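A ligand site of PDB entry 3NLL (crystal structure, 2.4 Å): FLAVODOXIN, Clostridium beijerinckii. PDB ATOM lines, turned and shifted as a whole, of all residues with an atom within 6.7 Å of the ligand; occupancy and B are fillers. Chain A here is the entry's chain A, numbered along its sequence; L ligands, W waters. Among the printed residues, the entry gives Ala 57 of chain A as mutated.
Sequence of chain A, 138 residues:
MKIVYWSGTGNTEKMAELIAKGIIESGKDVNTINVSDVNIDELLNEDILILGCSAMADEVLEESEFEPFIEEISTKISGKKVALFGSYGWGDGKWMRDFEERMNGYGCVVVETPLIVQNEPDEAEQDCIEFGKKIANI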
ATOM      1  N   TRP A   6      -1.374   1.046  22.834  1.00  0.00           N
ATOM      2  CA  TRP A   6      -0.570   0.369  23.858  1.00  0.00           C
ATOM      3  C   TRP A   6      -0.342   1.466  24.888  1.00  0.00           C
ATOM      4  O   TRP A   6      -0.100   2.623  24.508  1.00  0.00           O
ATOM      5  CB  TRP A   6       0.800  -0.097  23.330  1.00  0.00           C
ATOM      6  CG  TRP A   6       1.576  -0.808  24.423  1.00  0.00           C
ATOM      7  CD1 TRP A   6       1.441  -2.117  24.794  1.00  0.00           C
ATOM      8  CD2 TRP A   6       2.457  -0.216  25.396  1.00  0.00           C
ATOM      9  NE1 TRP A   6       2.147  -2.367  25.946  1.00  0.00           N
ATOM     10  CE2 TRP A   6       2.784  -1.221  26.338  1.00  0.00           C
ATOM     11  CE3 TRP A   6       2.997   1.076  25.567  1.00  0.00           C
ATOM     12  CZ2 TRP A   6       3.629  -0.983  27.439  1.00  0.00           C
ATOM     13  CZ3 TRP A   6       3.846   1.314  26.681  1.00  0.00           C
ATOM     14  CH2 TRP A   6       4.143   0.288  27.588  1.00  0.00           C
ATOM     15  N   SER A   7      -0.465   1.141  26.176  1.00  0.00           N
ATOM     16  CA  SER A   7      -0.230   2.122  27.223  1.00  0.00           C
ATOM     17  C   SER A   7       0.399   1.460  28.442  1.00  0.00           C
ATOM     18  O   SER A   7      -0.112   0.457  28.948  1.00  0.00           O
ATOM     19  CB  SER A   7      -1.535   2.820  27.584  1.00  0.00           C
ATOM     20  OG  SER A   7      -1.333   3.845  28.550  1.00  0.00           O
ATOM     21  N   GLY A   8       1.504   2.015  28.921  1.00  0.00           N
ATOM     22  CA  GLY A   8       2.184   1.441  30.064  1.00  0.00           C
ATOM     23  C   GLY A   8       1.724   1.926  31.427  1.00  0.00           C
ATOM     24  O   GLY A   8       1.878   1.213  32.427  1.00  0.00           O
ATOM     25  N   THR A   9       1.235   3.155  31.496  1.00  0.00           N
ATOM     26  CA  THR A   9       0.764   3.710  32.763  1.00  0.00           C
ATOM     27  C   THR A   9      -0.676   4.224  32.633  1.00  0.00           C
ATOM     28  O   THR A   9      -1.275   4.669  33.624  1.00  0.00           O
ATOM     29  CB  THR A   9       1.712   4.848  33.334  1.00  0.00           C
ATOM     30  OG1 THR A   9       1.498   6.078  32.623  1.00  0.00           O
ATOM     31  CG2 THR A   9       3.176   4.466  33.225  1.00  0.00           C
ATOM     32  N   GLY A  10      -1.230   4.179  31.415  1.00  0.00           N
ATOM     33  CA  GLY A  10      -2.586   4.626  31.199  1.00  0.00           C
ATOM     34  C   GLY A  10      -2.775   5.973  30.541  1.00  0.00           C
ATOM     35  O   GLY A  10      -3.899   6.388  30.320  1.00  0.00           O
ATOM     36  N   ASN A  11      -1.686   6.650  30.182  1.00  0.00           N
ATOM     37  CA  ASN A  11      -1.810   7.965  29.574  1.00  0.00           C
ATOM     38  C   ASN A  11      -2.413   7.912  28.179  1.00  0.00           C
ATOM     39  O   ASN A  11      -3.344   8.685  27.883  1.00  0.00           O
ATOM     40  CB  ASN A  11      -0.466   8.684  29.540  1.00  0.00           C
ATOM     41  CG  ASN A  11      -0.007   9.110  30.907  1.00  0.00           C
ATOM     42  OD1 ASN A  11       1.159   9.417  31.101  1.00  0.00           O
ATOM     43  ND2 ASN A  11      -0.920   9.139  31.864  1.00  0.00           N
ATOM     44  N   THR A  12      -1.863   7.035  27.337  1.00  0.00           N
ATOM     45  CA  THR A  12      -2.352   6.845  25.968  1.00  0.00           C
ATOM     46  C   THR A  12      -3.722   6.199  26.014  1.00  0.00           C
ATOM     47  O   THR A  12      -4.592   6.490  25.184  1.00  0.00           O
ATOM     48  CB  THR A  12      -1.394   5.949  25.160  1.00  0.00           C
ATOM     49  OG1 THR A  12      -0.082   6.525  25.199  1.00  0.00           O
ATOM     50  CG2 THR A  12      -1.835   5.863  23.700  1.00  0.00           C
ATOM     51  N   GLU A  13      -3.944   5.327  26.992  1.00  0.00           N
ATOM     52  CA  GLU A  13      -5.238   4.704  27.149  1.00  0.00           C
ATOM     53  C   GLU A  13      -6.294   5.800  27.343  1.00  0.00           C
ATOM     54  O   GLU A  13      -7.328   5.800  26.675  1.00  0.00           O
ATOM     55  CB  GLU A  13      -5.242   3.747  28.328  1.00  0.00           C
ATOM     56  CG  GLU A  13      -6.556   2.991  28.458  1.00  0.00           C
ATOM     57  CD  GLU A  13      -6.546   1.901  29.514  1.00  0.00           C
ATOM     58  OE1 GLU A  13      -5.861   2.059  30.552  1.00  0.00           O
ATOM     59  OE2 GLU A  13      -7.230   0.878  29.313  1.00  0.00           O
ATOM     60  N   LYS A  14      -6.009   6.779  28.200  1.00  0.00           N
ATOM     61  CA  LYS A  14      -6.950   7.882  28.436  1.00  0.00           C
ATOM     62  C   LYS A  14      -7.175   8.682  27.151  1.00  0.00           C
ATOM     63  O   LYS A  14      -8.302   9.068  26.851  1.00  0.00           O
ATOM     64  CB  LYS A  14      -6.488   8.809  29.547  1.00  0.00           C
ATOM     65  CG  LYS A  14      -7.596   9.765  30.005  1.00  0.00           C
ATOM     66  CD  LYS A  14      -7.119  10.767  31.057  1.00  0.00           C
ATOM     67  CE  LYS A  14      -8.203  11.790  31.417  1.00  0.00           C
ATOM     68  NZ  LYS A  14      -7.636  12.964  32.165  1.00  0.00           N
ATOM     69  N   CYS A  53       0.476   4.936  20.699  1.00  0.00           N
ATOM     70  CA  CYS A  53       1.464   4.308  21.546  1.00  0.00           C
ATOM     71  C   CYS A  53       2.359   5.396  22.082  1.00  0.00           C
ATOM     72  O   CYS A  53       2.707   6.337  21.367  1.00  0.00           O
ATOM     73  CB  CYS A  53       2.313   3.320  20.757  1.00  0.00           C
ATOM     74  SG  CYS A  53       3.624   2.489  21.707  1.00  0.00           S
ATOM     75  N   SER A  54       2.667   5.280  23.368  1.00  0.00           N
ATOM     76  CA  SER A  54       3.532   6.225  24.051  1.00  0.00           C
ATOM     77  C   SER A  54       4.985   6.069  23.590  1.00  0.00           C
ATOM     78  O   SER A  54       5.330   5.076  22.927  1.00  0.00           O
ATOM     79  CB  SER A  54       3.410   6.021  25.569  1.00  0.00           C
ATOM     80  OG  SER A  54       3.714   4.693  25.937  1.00  0.00           O
ATOM     81  N   ALA A  55       5.821   7.056  23.927  1.00  0.00           N
ATOM     82  CA  ALA A  55       7.224   7.051  23.539  1.00  0.00           C
ATOM     83  C   ALA A  55       8.083   6.203  24.468  1.00  0.00           C
ATOM     84  O   ALA A  55       8.101   6.439  25.665  1.00  0.00           O
ATOM     85  CB  ALA A  55       7.749   8.470  23.503  1.00  0.00           C
ATOM     86  N   MET A  56       8.748   5.195  23.922  1.00  0.00           N
ATOM     87  CA  MET A  56       9.635   4.365  24.725  1.00  0.00           C
ATOM     88  C   MET A  56      11.092   4.668  24.346  1.00  0.00           C
ATOM     89  O   MET A  56      11.348   5.430  23.421  1.00  0.00           O
ATOM     90  CB  MET A  56       9.305   2.880  24.555  1.00  0.00           C
ATOM     91  CG  MET A  56       7.976   2.458  25.183  1.00  0.00           C
ATOM     92  SD  MET A  56       7.902   2.712  26.977  1.00  0.00           S
ATOM     93  CE  MET A  56       6.644   3.964  27.103  1.00  0.00           C
ATOM     94  N   ALA A  57      12.042   4.100  25.084  1.00  0.00           N
ATOM     95  CA  ALA A  57      13.457   4.378  24.857  1.00  0.00           C
ATOM     96  C   ALA A  57      14.074   3.779  23.610  1.00  0.00           C
ATOM     97  O   ALA A  57      13.938   2.582  23.360  1.00  0.00           O
ATOM     98  CB  ALA A  57      14.256   3.938  26.094  1.00  0.00           C
ATOM     99  N   ASP A  58      14.688   4.607  22.767  1.00  0.00           N
ATOM    100  CA  ASP A  58      14.758   6.045  22.959  1.00  0.00           C
ATOM    101  C   ASP A  58      14.054   6.618  21.772  1.00  0.00           C
ATOM    102  O   ASP A  58      14.513   6.505  20.644  1.00  0.00           O
ATOM    103  CB  ASP A  58      16.204   6.523  22.958  1.00  0.00           C
ATOM    104  CG  ASP A  58      16.813   6.497  24.333  1.00  0.00           C
ATOM    105  OD1 ASP A  58      16.288   7.211  25.219  1.00  0.00           O
ATOM    106  OD2 ASP A  58      17.818   5.755  24.526  1.00  0.00           O
ATOM    107  N   GLU A  59      12.887   7.190  22.041  1.00  0.00           N
ATOM    108  CA  GLU A  59      12.038   7.761  21.011  1.00  0.00           C
ATOM    109  C   GLU A  59      11.653   6.704  19.980  1.00  0.00           C
ATOM    110  O   GLU A  59      11.736   6.969  18.764  1.00  0.00           O
ATOM    111  CB  GLU A  59      12.711   8.962  20.349  1.00  0.00           C
ATOM    112  CG  GLU A  59      12.947  10.155  21.269  1.00  0.00           C
ATOM    113  CD  GLU A  59      11.669  10.783  21.839  1.00  0.00           C
ATOM    114  OE1 GLU A  59      10.554  10.548  21.342  1.00  0.00           O
ATOM    115  OE2 GLU A  59      11.804  11.560  22.804  1.00  0.00           O
ATOM    116  N   VAL A  60      11.235   5.538  20.467  1.00  0.00           N
ATOM    117  CA  VAL A  60      10.813   4.428  19.609  1.00  0.00           C
ATOM    118  C   VAL A  60       9.460   3.916  20.078  1.00  0.00           C
ATOM    119  O   VAL A  60       9.004   4.282  21.166  1.00  0.00           O
ATOM    120  CB  VAL A  60      11.812   3.220  19.619  1.00  0.00           C
ATOM    121  CG1 VAL A  60      13.183   3.657  19.111  1.00  0.00           C
ATOM    122  CG2 VAL A  60      11.917   2.609  21.003  1.00  0.00           C
ATOM    123  N   GLY A  86      -0.459   9.653  20.665  1.00  0.00           N
ATOM    124  CA  GLY A  86       0.339   9.053  21.710  1.00  0.00           C
ATOM    125  C   GLY A  86       0.779  10.063  22.743  1.00  0.00           C
ATOM    126  O   GLY A  86       0.790  11.267  22.498  1.00  0.00           O
ATOM    127  N   SER A  87       1.172   9.563  23.911  1.00  0.00           N
ATOM    128  CA  SER A  87       1.612  10.392  25.017  1.00  0.00           C
ATOM    129  C   SER A  87       3.126  10.251  25.104  1.00  0.00           C
ATOM    130  O   SER A  87       3.684   9.225  24.706  1.00  0.00           O
ATOM    131  CB  SER A  87       0.927   9.912  26.299  1.00  0.00           C
ATOM    132  OG  SER A  87       1.366  10.611  27.448  1.00  0.00           O
ATOM    133  N   TYR A  88       3.805  11.289  25.577  1.00  0.00           N
ATOM    134  CA  TYR A  88       5.263  11.239  25.712  1.00  0.00           C
ATOM    135  C   TYR A  88       5.688  11.965  26.982  1.00  0.00           C
ATOM    136  O   TYR A  88       4.873  12.641  27.619  1.00  0.00           O
ATOM    137  CB  TYR A  88       5.966  11.814  24.481  1.00  0.00           C
ATOM    138  CG  TYR A  88       5.743  13.286  24.297  1.00  0.00           C
ATOM    139  CD1 TYR A  88       4.491  13.780  23.925  1.00  0.00           C
ATOM    140  CD2 TYR A  88       6.769  14.205  24.534  1.00  0.00           C
ATOM    141  CE1 TYR A  88       4.256  15.136  23.802  1.00  0.00           C
ATOM    142  CE2 TYR A  88       6.549  15.577  24.412  1.00  0.00           C
ATOM    143  CZ  TYR A  88       5.286  16.042  24.044  1.00  0.00           C
ATOM    144  OH  TYR A  88       5.036  17.390  23.947  1.00  0.00           O
ATOM    145  N   GLY A  89       6.951  11.826  27.351  1.00  0.00           N
ATOM    146  CA  GLY A  89       7.423  12.438  28.568  1.00  0.00           C
ATOM    147  C   GLY A  89       8.349  13.619  28.409  1.00  0.00           C
ATOM    148  O   GLY A  89       7.906  14.760  28.308  1.00  0.00           O
ATOM    149  N   TRP A  90       9.637  13.343  28.307  1.00  0.00           N
ATOM    150  CA  TRP A  90      10.630  14.399  28.216  1.00  0.00           C
ATOM    151  C   TRP A  90      11.090  14.814  26.823  1.00  0.00           C
ATOM    152  O   TRP A  90      11.774  15.819  26.687  1.00  0.00           O
ATOM    153  CB  TRP A  90      11.846  14.013  29.063  1.00  0.00           C
ATOM    154  CG  TRP A  90      12.426  12.682  28.672  1.00  0.00           C
ATOM    155  CD1 TRP A  90      13.306  12.438  27.661  1.00  0.00           C
ATOM    156  CD2 TRP A  90      12.112  11.396  29.253  1.00  0.00           C
ATOM    157  NE1 TRP A  90      13.562  11.100  27.572  1.00  0.00           N
ATOM    158  CE2 TRP A  90      12.837  10.438  28.527  1.00  0.00           C
ATOM    159  CE3 TRP A  90      11.276  10.979  30.295  1.00  0.00           C
ATOM    160  CZ2 TRP A  90      12.768   9.070  28.824  1.00  0.00           C
ATOM    161  CZ3 TRP A  90      11.209   9.616  30.583  1.00  0.00           C
ATOM    162  CH2 TRP A  90      11.952   8.679  29.851  1.00  0.00           C
ATOM    163  N   GLY A  91      10.726  14.063  25.788  1.00  0.00           N
ATOM    164  CA  GLY A  91      11.165  14.384  24.441  1.00  0.00           C
ATOM    165  C   GLY A  91      10.412  15.486  23.722  1.00  0.00           C
ATOM    166  O   GLY A  91       9.613  16.203  24.317  1.00  0.00           O
ATOM    167  N   ASP A  92      10.675  15.620  22.425  1.00  0.00           N
ATOM    168  CA  ASP A  92       9.994  16.619  21.595  1.00  0.00           C
ATOM    169  C   ASP A  92       9.135  15.993  20.501  1.00  0.00           C
ATOM    170  O   ASP A  92       8.822  16.642  19.495  1.00  0.00           O
ATOM    171  CB  ASP A  92      10.977  17.670  21.015  1.00  0.00           C
ATOM    172  CG  ASP A  92      11.986  17.082  20.034  1.00  0.00           C
ATOM    173  OD1 ASP A  92      11.647  16.177  19.240  1.00  0.00           O
ATOM    174  OD2 ASP A  92      13.136  17.573  20.019  1.00  0.00           O
ATOM    175  N   GLY A  93       8.788  14.720  20.657  1.00  0.00           N
ATOM    176  CA  GLY A  93       7.946  14.066  19.684  1.00  0.00           C
ATOM    177  C   GLY A  93       8.615  13.296  18.569  1.00  0.00           C
ATOM    178  O   GLY A  93       7.937  12.833  17.653  1.00  0.00           O
ATOM    179  N   TRP A  95       9.637  10.248  18.370  1.00  0.00           N
ATOM    180  CA  TRP A  95       9.088   8.917  18.137  1.00  0.00           C
ATOM    181  C   TRP A  95       7.858   9.016  17.247  1.00  0.00           C
ATOM    182  O   TRP A  95       7.597   8.125  16.438  1.00  0.00           O
ATOM    183  CB  TRP A  95       8.771   8.209  19.473  1.00  0.00           C
ATOM    184  CG  TRP A  95       7.306   8.163  19.858  1.00  0.00           C
ATOM    185  CD1 TRP A  95       6.476   7.063  19.817  1.00  0.00           C
ATOM    186  CD2 TRP A  95       6.508   9.251  20.348  1.00  0.00           C
ATOM    187  NE1 TRP A  95       5.217   7.405  20.247  1.00  0.00           N
ATOM    188  CE2 TRP A  95       5.210   8.740  20.582  1.00  0.00           C
ATOM    189  CE3 TRP A  95       6.763  10.600  20.618  1.00  0.00           C
ATOM    190  CZ2 TRP A  95       4.166   9.534  21.072  1.00  0.00           C
ATOM    191  CZ3 TRP A  95       5.729  11.393  21.099  1.00  0.00           C
ATOM    192  CH2 TRP A  95       4.446  10.855  21.321  1.00  0.00           C
ATOM    193  N   VAL A 117       0.456  14.322  23.344  1.00  0.00           N
ATOM    194  CA  VAL A 117       0.328  15.110  24.558  1.00  0.00           C
ATOM    195  C   VAL A 117       1.338  14.600  25.556  1.00  0.00           C
ATOM    196  O   VAL A 117       1.687  13.419  25.531  1.00  0.00           O
ATOM    197  CB  VAL A 117      -1.104  15.147  25.173  1.00  0.00           C
ATOM    198  CG1 VAL A 117      -2.148  15.031  24.093  1.00  0.00           C
ATOM    199  CG2 VAL A 117      -1.282  14.119  26.241  1.00  0.00           C
ATOM    200  N   GLN A 118       1.848  15.518  26.375  1.00  0.00           N
ATOM    201  CA  GLN A 118       2.848  15.177  27.361  1.00  0.00           C
ATOM    202  C   GLN A 118       2.153  14.659  28.581  1.00  0.00           C
ATOM    203  O   GLN A 118       1.259  15.324  29.101  1.00  0.00           O
ATOM    204  CB  GLN A 118       3.685  16.399  27.717  1.00  0.00           C
ATOM    205  CG  GLN A 118       4.975  16.036  28.433  1.00  0.00           C
ATOM    206  CD  GLN A 118       5.864  17.220  28.747  1.00  0.00           C
ATOM    207  OE1 GLN A 118       6.824  17.089  29.508  1.00  0.00           O
ATOM    208  NE2 GLN A 118       5.563  18.369  28.166  1.00  0.00           N
ATOM    209  N   ASN A 119       2.575  13.481  29.027  1.00  0.00           N
ATOM    210  CA  ASN A 119       2.027  12.792  30.191  1.00  0.00           C
ATOM    211  C   ASN A 119       0.510  12.613  30.119  1.00  0.00           C
ATOM    212  O   ASN A 119      -0.006  12.336  29.040  1.00  0.00           O
ATOM    213  CB  ASN A 119       2.504  13.462  31.493  1.00  0.00           C
ATOM    214  CG  ASN A 119       4.017  13.632  31.522  1.00  0.00           C
ATOM    215  OD1 ASN A 119       4.770  12.644  31.561  1.00  0.00           O
ATOM    216  ND2 ASN A 119       4.466  14.871  31.464  1.00  0.00           N
ATOM    217  N   GLU A 120      -0.203  12.742  31.236  1.00  0.00           N
ATOM    218  CA  GLU A 120      -1.652  12.536  31.204  1.00  0.00           C
ATOM    219  C   GLU A 120      -2.390  13.654  30.488  1.00  0.00           C
ATOM    220  O   GLU A 120      -2.063  14.819  30.672  1.00  0.00           O
ATOM    221  CB  GLU A 120      -2.223  12.339  32.619  1.00  0.00           C
ATOM    222  CG  GLU A 120      -3.657  11.789  32.605  1.00  0.00           C
ATOM    223  CD  GLU A 120      -4.256  11.511  33.986  1.00  0.00           C
ATOM    224  OE1 GLU A 120      -3.524  11.054  34.890  1.00  0.00           O
ATOM    225  OE2 GLU A 120      -5.484  11.731  34.148  1.00  0.00           O
HETATM  226  N1  LIG L   1       9.202   9.866  26.818  1.00  0.00           N
HETATM  227  C1  LIG L   1       9.804  10.585  25.821  1.00  0.00           C
HETATM  228  O1  LIG L   1       9.411  11.686  25.567  1.00  0.00           O
HETATM  229  N2  LIG L   1      10.876  10.039  25.114  1.00  0.00           N
HETATM  230  C2  LIG L   1      11.423   8.817  25.381  1.00  0.00           C
HETATM  231  O2  LIG L   1      12.358   8.365  24.723  1.00  0.00           O
HETATM  232  C3  LIG L   1      10.795   8.057  26.489  1.00  0.00           C
HETATM  233  N3  LIG L   1      11.302   6.911  26.874  1.00  0.00           N
HETATM  234  C4  LIG L   1      10.675   6.198  27.915  1.00  0.00           C
HETATM  235  C5  LIG L   1      11.172   4.925  28.293  1.00  0.00           C
HETATM  236  C6  LIG L   1      10.581   4.213  29.308  1.00  0.00           C
HETATM  237  C7  LIG L   1      11.206   2.933  29.784  1.00  0.00           C
HETATM  238  C8  LIG L   1       9.394   4.730  29.938  1.00  0.00           C
HETATM  239  C9  LIG L   1       8.670   3.949  31.015  1.00  0.00           C
HETATM  240  C10 LIG L   1       8.884   5.958  29.565  1.00  0.00           C
HETATM  241  C11 LIG L   1       9.513   6.708  28.560  1.00  0.00           C
HETATM  242  N4  LIG L   1       9.049   7.964  28.158  1.00  0.00           N
HETATM  243  C12 LIG L   1       9.643   8.682  27.134  1.00  0.00           C
HETATM  244  C13 LIG L   1       7.913   8.546  28.866  1.00  0.00           C
HETATM  245  C14 LIG L   1       6.567   8.034  28.371  1.00  0.00           C
HETATM  246  O3  LIG L   1       6.488   8.191  26.955  1.00  0.00           O
HETATM  247  C15 LIG L   1       5.462   8.837  29.040  1.00  0.00           C
HETATM  248  O4  LIG L   1       5.614   8.746  30.448  1.00  0.00           O
HETATM  249  C16 LIG L   1       4.004   8.631  28.681  1.00  0.00           C
HETATM  250  O5  LIG L   1       3.200   9.601  29.376  1.00  0.00           O
HETATM  251  C17 LIG L   1       3.578   7.196  28.968  1.00  0.00           C
HETATM  252  O6  LIG L   1       2.286   6.997  28.460  1.00  0.00           O
HETATM  253  P1  LIG L   1       1.609   5.612  28.661  1.00  0.00           P
HETATM  254  O7  LIG L   1       2.594   4.568  28.499  1.00  0.00           O
HETATM  255  O8  LIG L   1       0.458   5.591  27.761  1.00  0.00           O
HETATM  256  O9  LIG L   1       1.082   5.583  30.130  1.00  0.00           O
HETATM  257  O   HOH W   1       4.215  10.265  32.210  1.00  0.00           O
HETATM  258  O   HOH W   2       8.905  12.432  22.372  1.00  0.00           O
HETATM  259  O   HOH W   3       4.700   3.808  30.180  1.00  0.00           O
HETATM  260  O   HOH W   4       5.746   6.121  31.388  1.00  0.00           O
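Water W1 lies within hydrogen-bond range of the side-chain amide oxygen of Asn 119 (2.5 Å), an oxygen (O4) of the ligand (2.7 Å) and the side-chain amide oxygen of Asn 11 (3.4 Å).
Water W2 lies within hydrogen-bond range of the side-chain carboxylate of Glu 59 (2.7 Å), the backbone NH of Gly 93 (2.9 Å) and an oxygen (O1) of the ligand (3.3 Å).
The backbone NH of Gly 89 lies within hydrogen-bond range of a nitrogen (N1) of the ligand, 3.0 Å away.
The side-chain carboxylate (OE2) of Glu 59 sits at hydrogen-bond distance from a nitrogen (N2) of the ligand.
N of Thr 12 sits at hydrogen-bond distance from O8 of the ligand (2.8 Å).
The side-chain hydroxyl (OG1) of Thr 9 lies within hydrogen-bond range of an oxygen (O9) of the ligand.
O7 of the ligand sits at hydrogen-bond distance from N of Gly 8, at 2.8 Å.
The backbone NH of Gly 10 lies within hydrogen-bond range of an oxygen (O9) of the ligand (3.0 Å).
O5 of the ligand lies within hydrogen-bond range of OD1 of Asn 11 (2.7 Å).
The side-chain hydroxyl (OG) of Ser 7 sits at hydrogen-bond distance from an oxygen (O8) of the ligand, 2.6 Å away.
The side-chain hydroxyl (OG1) of Thr 12 sits at hydrogen-bond distance from an oxygen (O8) of the ligand (2.8 Å).
An oxygen (O3) of the ligand sits at hydrogen-bond distance from the backbone NH (N) of Ala 55, 3.3 Å away.
An oxygen (O9) of the ligand sits at hydrogen-bond distance from the backbone NH (N) of Asn 11 (3.0 Å).
O5 of the ligand is in hydrogen-bond range of OG of Ser 87.
The backbone NH (N) of Gly 91 sits at hydrogen-bond distance from an oxygen (O1) of the ligand (2.7 Å).
The backbone carbonyl oxygen (O) of Ala 55 is in hydrogen-bond range of an oxygen (O3) of the ligand (2.7 Å).
The side-chain hydroxyl (OG) of Ser 54 sits at hydrogen-bond distance from an oxygen (O7) of the ligand (2.8 Å).
O9 of the ligand sits at hydrogen-bond distance from N of Thr 9, 2.8 Å away.
An oxygen (O2) of the ligand lies within hydrogen-bond range of the backbone NH (N) of Glu 59 (3.0 Å).
The backbone NH (N) of Trp 90 is in hydrogen-bond range of an oxygen (O1) of the ligand.
The backbone NH (N) of Ala 57 sits at hydrogen-bond distance from a nitrogen (N3) of the ligand, at 3.4 Å.
OE1 of Glu 59 sits at hydrogen-bond distance from N of Trp 95, at 3.1 Å.
OG of Ser 7 is in hydrogen-bond range of N of Asn 11, 3.3 Å away.
OG of Ser 87 is in hydrogen-bond range of O of Asn 119 (2.7 Å).
O of Val 117 sits at hydrogen-bond distance from N of Tyr 88 (3.0 Å).
The side-chain hydroxyl (OG) of Ser 7 is in hydrogen-bond range of the backbone NH (N) of Thr 12 (3.5 Å).
The backbone carbonyl oxygen (O) of Tyr 88 sits at hydrogen-bond distance from the backbone NH (N) of Asn 119 (2.8 Å).
The side-chain hydroxyl of Ser 7 sits at hydrogen-bond distance from the backbone NH of Gly 10 (2.9 Å).
The backbone NH of Ala 55 lies within hydrogen-bond range of the backbone carbonyl oxygen of Ser 87, at 3.1 Å.
The backbone carbonyl oxygen (O) of Met 56 sits close to an oxygen (O2) of the ligand (3.4 Å).
Residues that only touch the ligand: Asn 119 (3.5 Å), Tyr 88 (3.5 Å), Asp 58 (3.8 Å) and Trp 6 (3.9 Å).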
